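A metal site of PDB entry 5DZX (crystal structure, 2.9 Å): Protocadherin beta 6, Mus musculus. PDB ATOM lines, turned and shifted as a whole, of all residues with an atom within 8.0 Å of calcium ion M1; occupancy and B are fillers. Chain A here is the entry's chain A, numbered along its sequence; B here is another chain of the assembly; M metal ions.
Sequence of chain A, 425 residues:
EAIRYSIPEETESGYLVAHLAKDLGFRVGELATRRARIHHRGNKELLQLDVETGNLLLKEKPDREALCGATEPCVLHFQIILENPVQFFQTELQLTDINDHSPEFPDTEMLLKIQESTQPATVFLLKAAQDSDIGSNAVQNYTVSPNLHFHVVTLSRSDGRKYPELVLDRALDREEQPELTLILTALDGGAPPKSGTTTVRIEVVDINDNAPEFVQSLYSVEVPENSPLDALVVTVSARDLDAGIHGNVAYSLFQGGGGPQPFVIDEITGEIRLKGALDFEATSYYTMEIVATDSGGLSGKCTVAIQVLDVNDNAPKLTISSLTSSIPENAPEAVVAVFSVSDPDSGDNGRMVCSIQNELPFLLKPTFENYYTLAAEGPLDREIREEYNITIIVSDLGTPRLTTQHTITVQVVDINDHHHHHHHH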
ATOM      1  N   GLU A 175       7.389 -18.097 -30.845  1.00  0.00           N
ATOM      2  CA  GLU A 175       7.542 -16.653 -30.771  1.00  0.00           C
ATOM      3  C   GLU A 175       7.845 -16.047 -32.139  1.00  0.00           C
ATOM      4  O   GLU A 175       7.457 -14.909 -32.420  1.00  0.00           O
ATOM      5  CB  GLU A 175       8.629 -16.280 -29.764  1.00  0.00           C
ATOM      6  CG  GLU A 175       8.184 -16.411 -28.309  1.00  0.00           C
ATOM      7  CD  GLU A 175       7.897 -17.841 -27.894  1.00  0.00           C
ATOM      8  OE1 GLU A 175       8.489 -18.769 -28.495  1.00  0.00           O
ATOM      9  OE2 GLU A 175       7.061 -18.053 -26.992  1.00  0.00           O
ATOM     10  N   ASP A 206       2.285 -23.542 -27.335  1.00  0.00           N
ATOM     11  CA  ASP A 206       3.051 -22.654 -26.460  1.00  0.00           C
ATOM     12  C   ASP A 206       3.558 -23.394 -25.235  1.00  0.00           C
ATOM     13  O   ASP A 206       2.793 -24.082 -24.552  1.00  0.00           O
ATOM     14  CB  ASP A 206       2.198 -21.457 -26.028  1.00  0.00           C
ATOM     15  CG  ASP A 206       2.988 -20.456 -25.190  1.00  0.00           C
ATOM     16  OD1 ASP A 206       4.221 -20.342 -25.400  1.00  0.00           O
ATOM     17  OD2 ASP A 206       2.380 -19.789 -24.324  1.00  0.00           O
ATOM     18  N   ILE A 207       4.849 -23.276 -24.980  1.00  0.00           N
ATOM     19  CA  ILE A 207       5.442 -23.818 -23.774  1.00  0.00           C
ATOM     20  C   ILE A 207       6.151 -22.714 -23.012  1.00  0.00           C
ATOM     21  O   ILE A 207       6.352 -21.622 -23.531  1.00  0.00           O
ATOM     22  CB  ILE A 207       6.426 -24.971 -24.088  1.00  0.00           C
ATOM     23  CG1 ILE A 207       7.578 -24.465 -24.948  1.00  0.00           C
ATOM     24  CG2 ILE A 207       5.696 -26.125 -24.763  1.00  0.00           C
ATOM     25  CD1 ILE A 207       8.912 -24.523 -24.244  1.00  0.00           C
ATOM     26  N   ASN A 208       6.517 -23.011 -21.777  1.00  0.00           N
ATOM     27  CA  ASN A 208       7.124 -22.009 -20.908  1.00  0.00           C
ATOM     28  C   ASN A 208       8.645 -21.962 -21.030  1.00  0.00           C
ATOM     29  O   ASN A 208       9.355 -22.669 -20.318  1.00  0.00           O
ATOM     30  CB  ASN A 208       6.716 -22.275 -19.468  1.00  0.00           C
ATOM     31  CG  ASN A 208       6.744 -21.030 -18.627  1.00  0.00           C
ATOM     32  OD1 ASN A 208       6.607 -19.919 -19.135  1.00  0.00           O
ATOM     33  ND2 ASN A 208       6.903 -21.197 -17.312  1.00  0.00           N
ATOM     34  N   ASP A 209       9.137 -21.110 -21.928  1.00  0.00           N
ATOM     35  CA  ASP A 209      10.570 -21.016 -22.169  1.00  0.00           C
ATOM     36  C   ASP A 209      11.093 -19.582 -22.098  1.00  0.00           C
ATOM     37  O   ASP A 209      12.294 -19.332 -22.265  1.00  0.00           O
ATOM     38  CB  ASP A 209      10.920 -21.639 -23.522  1.00  0.00           C
ATOM     39  CG  ASP A 209      10.056 -21.106 -24.645  1.00  0.00           C
ATOM     40  OD1 ASP A 209       8.903 -20.704 -24.383  1.00  0.00           O
ATOM     41  OD2 ASP A 209      10.512 -21.106 -25.809  1.00  0.00           O
ATOM     42  N   ASN A 210      10.198 -18.626 -21.845  1.00  0.00           N
ATOM     43  CA  ASN A 210      10.586 -17.227 -21.719  1.00  0.00           C
ATOM     44  C   ASN A 210      10.217 -16.637 -20.368  1.00  0.00           C
ATOM     45  O   ASN A 210       9.041 -16.554 -20.014  1.00  0.00           O
ATOM     46  CB  ASN A 210       9.961 -16.396 -22.839  1.00  0.00           C
ATOM     47  CG  ASN A 210      10.541 -16.713 -24.195  1.00  0.00           C
ATOM     48  OD1 ASN A 210      11.720 -17.050 -24.316  1.00  0.00           O
ATOM     49  ND2 ASN A 210       9.708 -16.627 -25.223  1.00  0.00           N
ATOM     50  N   ALA A 211      11.230 -16.207 -19.613  1.00  0.00           N
ATOM     51  CA  ALA A 211      10.990 -15.621 -18.296  1.00  0.00           C
ATOM     52  C   ALA A 211      10.437 -14.216 -18.439  1.00  0.00           C
ATOM     53  O   ALA A 211      10.810 -13.495 -19.369  1.00  0.00           O
ATOM     54  CB  ALA A 211      12.281 -15.619 -17.483  1.00  0.00           C
ATOM     55  N   PRO A 212       9.530 -13.821 -17.533  1.00  0.00           N
ATOM     56  CA  PRO A 212       8.996 -12.461 -17.545  1.00  0.00           C
ATOM     57  C   PRO A 212      10.082 -11.421 -17.235  1.00  0.00           C
ATOM     58  O   PRO A 212      10.830 -11.600 -16.284  1.00  0.00           O
ATOM     59  CB  PRO A 212       7.923 -12.485 -16.442  1.00  0.00           C
ATOM     60  CG  PRO A 212       8.344 -13.599 -15.542  1.00  0.00           C
ATOM     61  CD  PRO A 212       8.972 -14.633 -16.441  1.00  0.00           C
ATOM     62  N   GLU A 213      10.167 -10.371 -18.048  1.00  0.00           N
ATOM     63  CA  GLU A 213      11.182  -9.345 -17.854  1.00  0.00           C
ATOM     64  C   GLU A 213      10.549  -7.979 -17.548  1.00  0.00           C
ATOM     65  O   GLU A 213       9.464  -7.663 -18.037  1.00  0.00           O
ATOM     66  CB  GLU A 213      12.090  -9.243 -19.081  1.00  0.00           C
ATOM     67  CG  GLU A 213      13.340  -8.412 -18.865  1.00  0.00           C
ATOM     68  CD  GLU A 213      14.336  -8.552 -20.012  1.00  0.00           C
ATOM     69  OE1 GLU A 213      14.169  -9.479 -20.839  1.00  0.00           O
ATOM     70  OE2 GLU A 213      15.274  -7.726 -20.082  1.00  0.00           O
ATOM     71  N   ARG A 239       6.481  -7.781 -18.932  1.00  0.00           N
ATOM     72  CA  ARG A 239       5.870  -8.413 -20.095  1.00  0.00           C
ATOM     73  C   ARG A 239       6.414  -9.817 -20.296  1.00  0.00           C
ATOM     74  O   ARG A 239       7.597 -10.088 -20.072  1.00  0.00           O
ATOM     75  CB  ARG A 239       6.108  -7.581 -21.352  1.00  0.00           C
ATOM     76  CG  ARG A 239       5.750  -6.101 -21.210  1.00  0.00           C
ATOM     77  CD  ARG A 239       6.190  -5.317 -22.431  1.00  0.00           C
ATOM     78  NE  ARG A 239       5.404  -5.671 -23.612  1.00  0.00           N
ATOM     79  CZ  ARG A 239       5.714  -5.327 -24.856  1.00  0.00           C
ATOM     80  NH1 ARG A 239       6.813  -4.633 -25.099  1.00  0.00           N
ATOM     81  NH2 ARG A 239       4.930  -5.688 -25.865  1.00  0.00           N
ATOM     82  N   ASP A 240       5.542 -10.730 -20.712  1.00  0.00           N
ATOM     83  CA  ASP A 240       5.938 -12.110 -20.978  1.00  0.00           C
ATOM     84  C   ASP A 240       5.714 -12.466 -22.440  1.00  0.00           C
ATOM     85  O   ASP A 240       4.640 -12.240 -22.988  1.00  0.00           O
ATOM     86  CB  ASP A 240       5.168 -13.076 -20.080  1.00  0.00           C
ATOM     87  CG  ASP A 240       5.867 -14.407 -19.911  1.00  0.00           C
ATOM     88  OD1 ASP A 240       6.661 -14.767 -20.794  1.00  0.00           O
ATOM     89  OD2 ASP A 240       5.612 -15.078 -18.897  1.00  0.00           O
ATOM     90  N   LEU A 241       6.745 -13.033 -23.055  1.00  0.00           N
ATOM     91  CA  LEU A 241       6.677 -13.417 -24.469  1.00  0.00           C
ATOM     92  C   LEU A 241       5.693 -14.552 -24.707  1.00  0.00           C
ATOM     93  O   LEU A 241       5.073 -14.635 -25.770  1.00  0.00           O
ATOM     94  CB  LEU A 241       8.067 -13.804 -24.988  1.00  0.00           C
ATOM     95  CG  LEU A 241       9.110 -12.692 -25.095  1.00  0.00           C
ATOM     96  CD1 LEU A 241      10.413 -13.252 -25.641  1.00  0.00           C
ATOM     97  CD2 LEU A 241       8.596 -11.553 -25.968  1.00  0.00           C
ATOM     98  N   ASP A 242       5.559 -15.435 -23.715  1.00  0.00           N
ATOM     99  CA  ASP A 242       4.669 -16.590 -23.838  1.00  0.00           C
ATOM    100  C   ASP A 242       3.193 -16.175 -23.746  1.00  0.00           C
ATOM    101  O   ASP A 242       2.875 -15.041 -23.391  1.00  0.00           O
ATOM    102  CB  ASP A 242       4.995 -17.607 -22.751  1.00  0.00           C
ATOM    103  CG  ASP A 242       6.431 -18.080 -22.802  1.00  0.00           C
ATOM    104  OD1 ASP A 242       7.000 -18.158 -23.919  1.00  0.00           O
ATOM    105  OD2 ASP A 242       7.016 -18.361 -21.735  1.00  0.00           O
ATOM    106  N   ALA A 243       2.309 -17.108 -24.064  1.00  0.00           N
ATOM    107  CA  ALA A 243       0.874 -16.828 -24.038  1.00  0.00           C
ATOM    108  C   ALA A 243       0.155 -17.784 -23.092  1.00  0.00           C
ATOM    109  O   ALA A 243       0.737 -18.756 -22.607  1.00  0.00           O
ATOM    110  CB  ALA A 243       0.280 -16.910 -25.429  1.00  0.00           C
ATOM    111  N   ILE A 245      -1.400 -19.396 -19.849  1.00  0.00           N
ATOM    112  CA  ILE A 245      -0.982 -19.443 -18.453  1.00  0.00           C
ATOM    113  C   ILE A 245       0.522 -19.216 -18.344  1.00  0.00           C
ATOM    114  O   ILE A 245       1.036 -18.889 -17.273  1.00  0.00           O
ATOM    115  CB  ILE A 245      -1.358 -20.790 -17.786  1.00  0.00           C
ATOM    116  CG1 ILE A 245      -1.317 -20.670 -16.264  1.00  0.00           C
ATOM    117  CG2 ILE A 245      -0.457 -21.914 -18.298  1.00  0.00           C
ATOM    118  CD1 ILE A 245      -1.634 -21.973 -15.546  1.00  0.00           C
ATOM    119  N   HIS A 246       1.235 -19.391 -19.454  1.00  0.00           N
ATOM    120  CA  HIS A 246       2.672 -19.183 -19.491  1.00  0.00           C
ATOM    121  C   HIS A 246       2.992 -17.703 -19.686  1.00  0.00           C
ATOM    122  O   HIS A 246       4.157 -17.304 -19.623  1.00  0.00           O
ATOM    123  CB  HIS A 246       3.319 -20.009 -20.608  1.00  0.00           C
ATOM    124  CG  HIS A 246       2.842 -21.430 -20.666  1.00  0.00           C
ATOM    125  ND1 HIS A 246       3.167 -22.369 -19.709  1.00  0.00           N
ATOM    126  CD2 HIS A 246       2.086 -22.077 -21.580  1.00  0.00           C
ATOM    127  CE1 HIS A 246       2.622 -23.532 -20.026  1.00  0.00           C
ATOM    128  NE2 HIS A 246       1.955 -23.380 -21.160  1.00  0.00           N
ATOM    129  N   GLY A 247       1.957 -16.904 -19.920  1.00  0.00           N
ATOM    130  CA  GLY A 247       2.122 -15.482 -20.156  1.00  0.00           C
ATOM    131  C   GLY A 247       1.647 -14.616 -18.999  1.00  0.00           C
ATOM    132  O   GLY A 247       2.027 -13.446 -18.901  1.00  0.00           O
ATOM    133  N   ASN A 248       0.812 -15.184 -18.136  1.00  0.00           N
ATOM    134  CA  ASN A 248       0.300 -14.477 -16.966  1.00  0.00           C
ATOM    135  C   ASN A 248       1.408 -14.195 -15.954  1.00  0.00           C
ATOM    136  O   ASN A 248       2.263 -15.055 -15.712  1.00  0.00           O
ATOM    137  CB  ASN A 248      -0.823 -15.256 -16.308  1.00  0.00           C
ATOM    138  CG  ASN A 248      -2.106 -15.230 -17.112  1.00  0.00           C
ATOM    139  OD1 ASN A 248      -2.091 -15.001 -18.331  1.00  0.00           O
ATOM    140  ND2 ASN A 248      -3.235 -15.444 -16.442  1.00  0.00           N
ATOM    141  N   VAL A 249       1.375 -13.012 -15.355  1.00  0.00           N
ATOM    142  CA  VAL A 249       2.436 -12.603 -14.448  1.00  0.00           C
ATOM    143  C   VAL A 249       1.914 -12.336 -13.040  1.00  0.00           C
ATOM    144  O   VAL A 249       0.863 -11.726 -12.851  1.00  0.00           O
ATOM    145  CB  VAL A 249       3.145 -11.328 -14.991  1.00  0.00           C
ATOM    146  CG1 VAL A 249       2.133 -10.228 -15.280  1.00  0.00           C
ATOM    147  CG2 VAL A 249       4.210 -10.846 -14.027  1.00  0.00           C
ATOM    148  N   THR A 293       6.847 -13.385 -10.999  1.00  0.00           N
ATOM    149  CA  THR A 293       6.919 -14.827 -11.176  1.00  0.00           C
ATOM    150  C   THR A 293       5.880 -15.299 -12.181  1.00  0.00           C
ATOM    151  O   THR A 293       4.732 -14.858 -12.168  1.00  0.00           O
ATOM    152  CB  THR A 293       6.692 -15.571  -9.836  1.00  0.00           C
ATOM    153  OG1 THR A 293       7.615 -15.085  -8.862  1.00  0.00           O
ATOM    154  CG2 THR A 293       6.902 -17.075 -10.030  1.00  0.00           C
ATOM    155  N   ASP A 294       6.319 -16.173 -13.078  1.00  0.00           N
ATOM    156  CA  ASP A 294       5.420 -16.780 -14.044  1.00  0.00           C
ATOM    157  C   ASP A 294       4.591 -17.889 -13.390  1.00  0.00           C
ATOM    158  O   ASP A 294       4.947 -18.382 -12.322  1.00  0.00           O
ATOM    159  CB  ASP A 294       6.206 -17.332 -15.232  1.00  0.00           C
ATOM    160  CG  ASP A 294       5.331 -17.679 -16.399  1.00  0.00           C
ATOM    161  OD1 ASP A 294       4.152 -17.270 -16.400  1.00  0.00           O
ATOM    162  OD2 ASP A 294       5.825 -18.344 -17.333  1.00  0.00           O
ATOM    163  N   SER A 295       3.478 -18.250 -14.019  1.00  0.00           N
ATOM    164  CA  SER A 295       2.628 -19.315 -13.509  1.00  0.00           C
ATOM    165  C   SER A 295       3.281 -20.681 -13.675  1.00  0.00           C
ATOM    166  O   SER A 295       2.786 -21.688 -13.179  1.00  0.00           O
ATOM    167  CB  SER A 295       1.263 -19.301 -14.211  1.00  0.00           C
ATOM    168  OG  SER A 295       0.635 -18.038 -14.061  1.00  0.00           O
ATOM    169  N   GLY A 296       4.384 -20.704 -14.419  1.00  0.00           N
ATOM    170  CA  GLY A 296       5.180 -21.918 -14.573  1.00  0.00           C
ATOM    171  C   GLY A 296       6.291 -21.971 -13.543  1.00  0.00           C
ATOM    172  O   GLY A 296       6.544 -23.006 -12.933  1.00  0.00           O
ATOM    173  N   GLY A 297       6.951 -20.833 -13.330  1.00  0.00           N
ATOM    174  CA  GLY A 297       8.006 -20.755 -12.340  1.00  0.00           C
ATOM    175  C   GLY A 297       9.114 -19.786 -12.697  1.00  0.00           C
ATOM    176  O   GLY A 297       9.945 -19.435 -11.847  1.00  0.00           O
ATOM    177  N   LEU A 298       9.134 -19.343 -13.952  1.00  0.00           N
ATOM    178  CA  LEU A 298      10.150 -18.402 -14.399  1.00  0.00           C
ATOM    179  C   LEU A 298       9.940 -17.041 -13.745  1.00  0.00           C
ATOM    180  O   LEU A 298       8.806 -16.608 -13.546  1.00  0.00           O
ATOM    181  CB  LEU A 298      10.137 -18.279 -15.920  1.00  0.00           C
ATOM    182  CG  LEU A 298      10.271 -19.581 -16.697  1.00  0.00           C
ATOM    183  CD1 LEU A 298      10.362 -19.303 -18.193  1.00  0.00           C
ATOM    184  CD2 LEU A 298      11.469 -20.406 -16.221  1.00  0.00           C
ATOM    185  N   SER A 299      11.034 -16.365 -13.416  1.00  0.00           N
ATOM    186  CA  SER A 299      10.937 -15.111 -12.662  1.00  0.00           C
ATOM    187  C   SER A 299      11.869 -14.006 -13.175  1.00  0.00           C
ATOM    188  O   SER A 299      12.970 -14.279 -13.657  1.00  0.00           O
ATOM    189  CB  SER A 299      11.218 -15.380 -11.193  1.00  0.00           C
ATOM    190  OG  SER A 299      12.391 -16.169 -11.033  1.00  0.00           O
ATOM    191  N   GLN B 115       8.062 -25.146 -12.139  1.00  0.00           N
ATOM    192  CA  GLN B 115       7.680 -26.111 -13.172  1.00  0.00           C
ATOM    193  C   GLN B 115       8.590 -27.329 -13.171  1.00  0.00           C
ATOM    194  O   GLN B 115       9.763 -27.256 -12.791  1.00  0.00           O
ATOM    195  CB  GLN B 115       7.681 -25.454 -14.552  1.00  0.00           C
ATOM    196  CG  GLN B 115       9.042 -25.028 -15.058  1.00  0.00           C
ATOM    197  CD  GLN B 115       8.977 -24.329 -16.395  1.00  0.00           C
ATOM    198  OE1 GLN B 115       7.902 -23.946 -16.857  1.00  0.00           O
ATOM    199  NE2 GLN B 115      10.128 -24.168 -17.042  1.00  0.00           N
HETATM  200 CA    CA M   1       6.837 -16.986 -19.158  1.00  0.00          CA
HETATM  201 CA    CA M   2       6.586 -20.013 -25.768  1.00  0.00          CA
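N of Asp 242 sits close to OD1 of Asp 240 (3.2 Å).
The backbone NH of Asn 210 lies within hydrogen-bond range of the side-chain carboxylate of Asp 242, 3.2 Å away.
OD1 of Asn 208 sits close to OD2 of Asp 294, at 2.5 Å.
OE1 of Gln 115 of chain B lies within hydrogen-bond range of ND2 of Asn 208 (3.0 Å).
The side-chain amide oxygen (OD1) of Asn 208 sits close to the side-chain carboxylate (OD2) of Asp 242, at 3.1 Å.
ND2 of Asn 210 lies close to OE2 of Glu 175 (3.5 Å).
Calcium ion M1 is bound by the side-chain carboxylate (OD2) of Asp 240, the backbone carbonyl oxygen (O) of Asn 210, the side-chain carboxylate (OD2) of Asp 294, the backbone carbonyl oxygen (O) of His 246 and the side-chain carboxylate (OD1) of Asp 240.
Slightly farther from calcium ion M1 lies OD2 of Asp 242 (2.9 Å).
Slightly farther from calcium ion M1 lies OD1 of Asn 208 (2.9 Å).
The nearest printed residue that does not touch calcium ion M1 is Pro 212 (4.2 Å).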
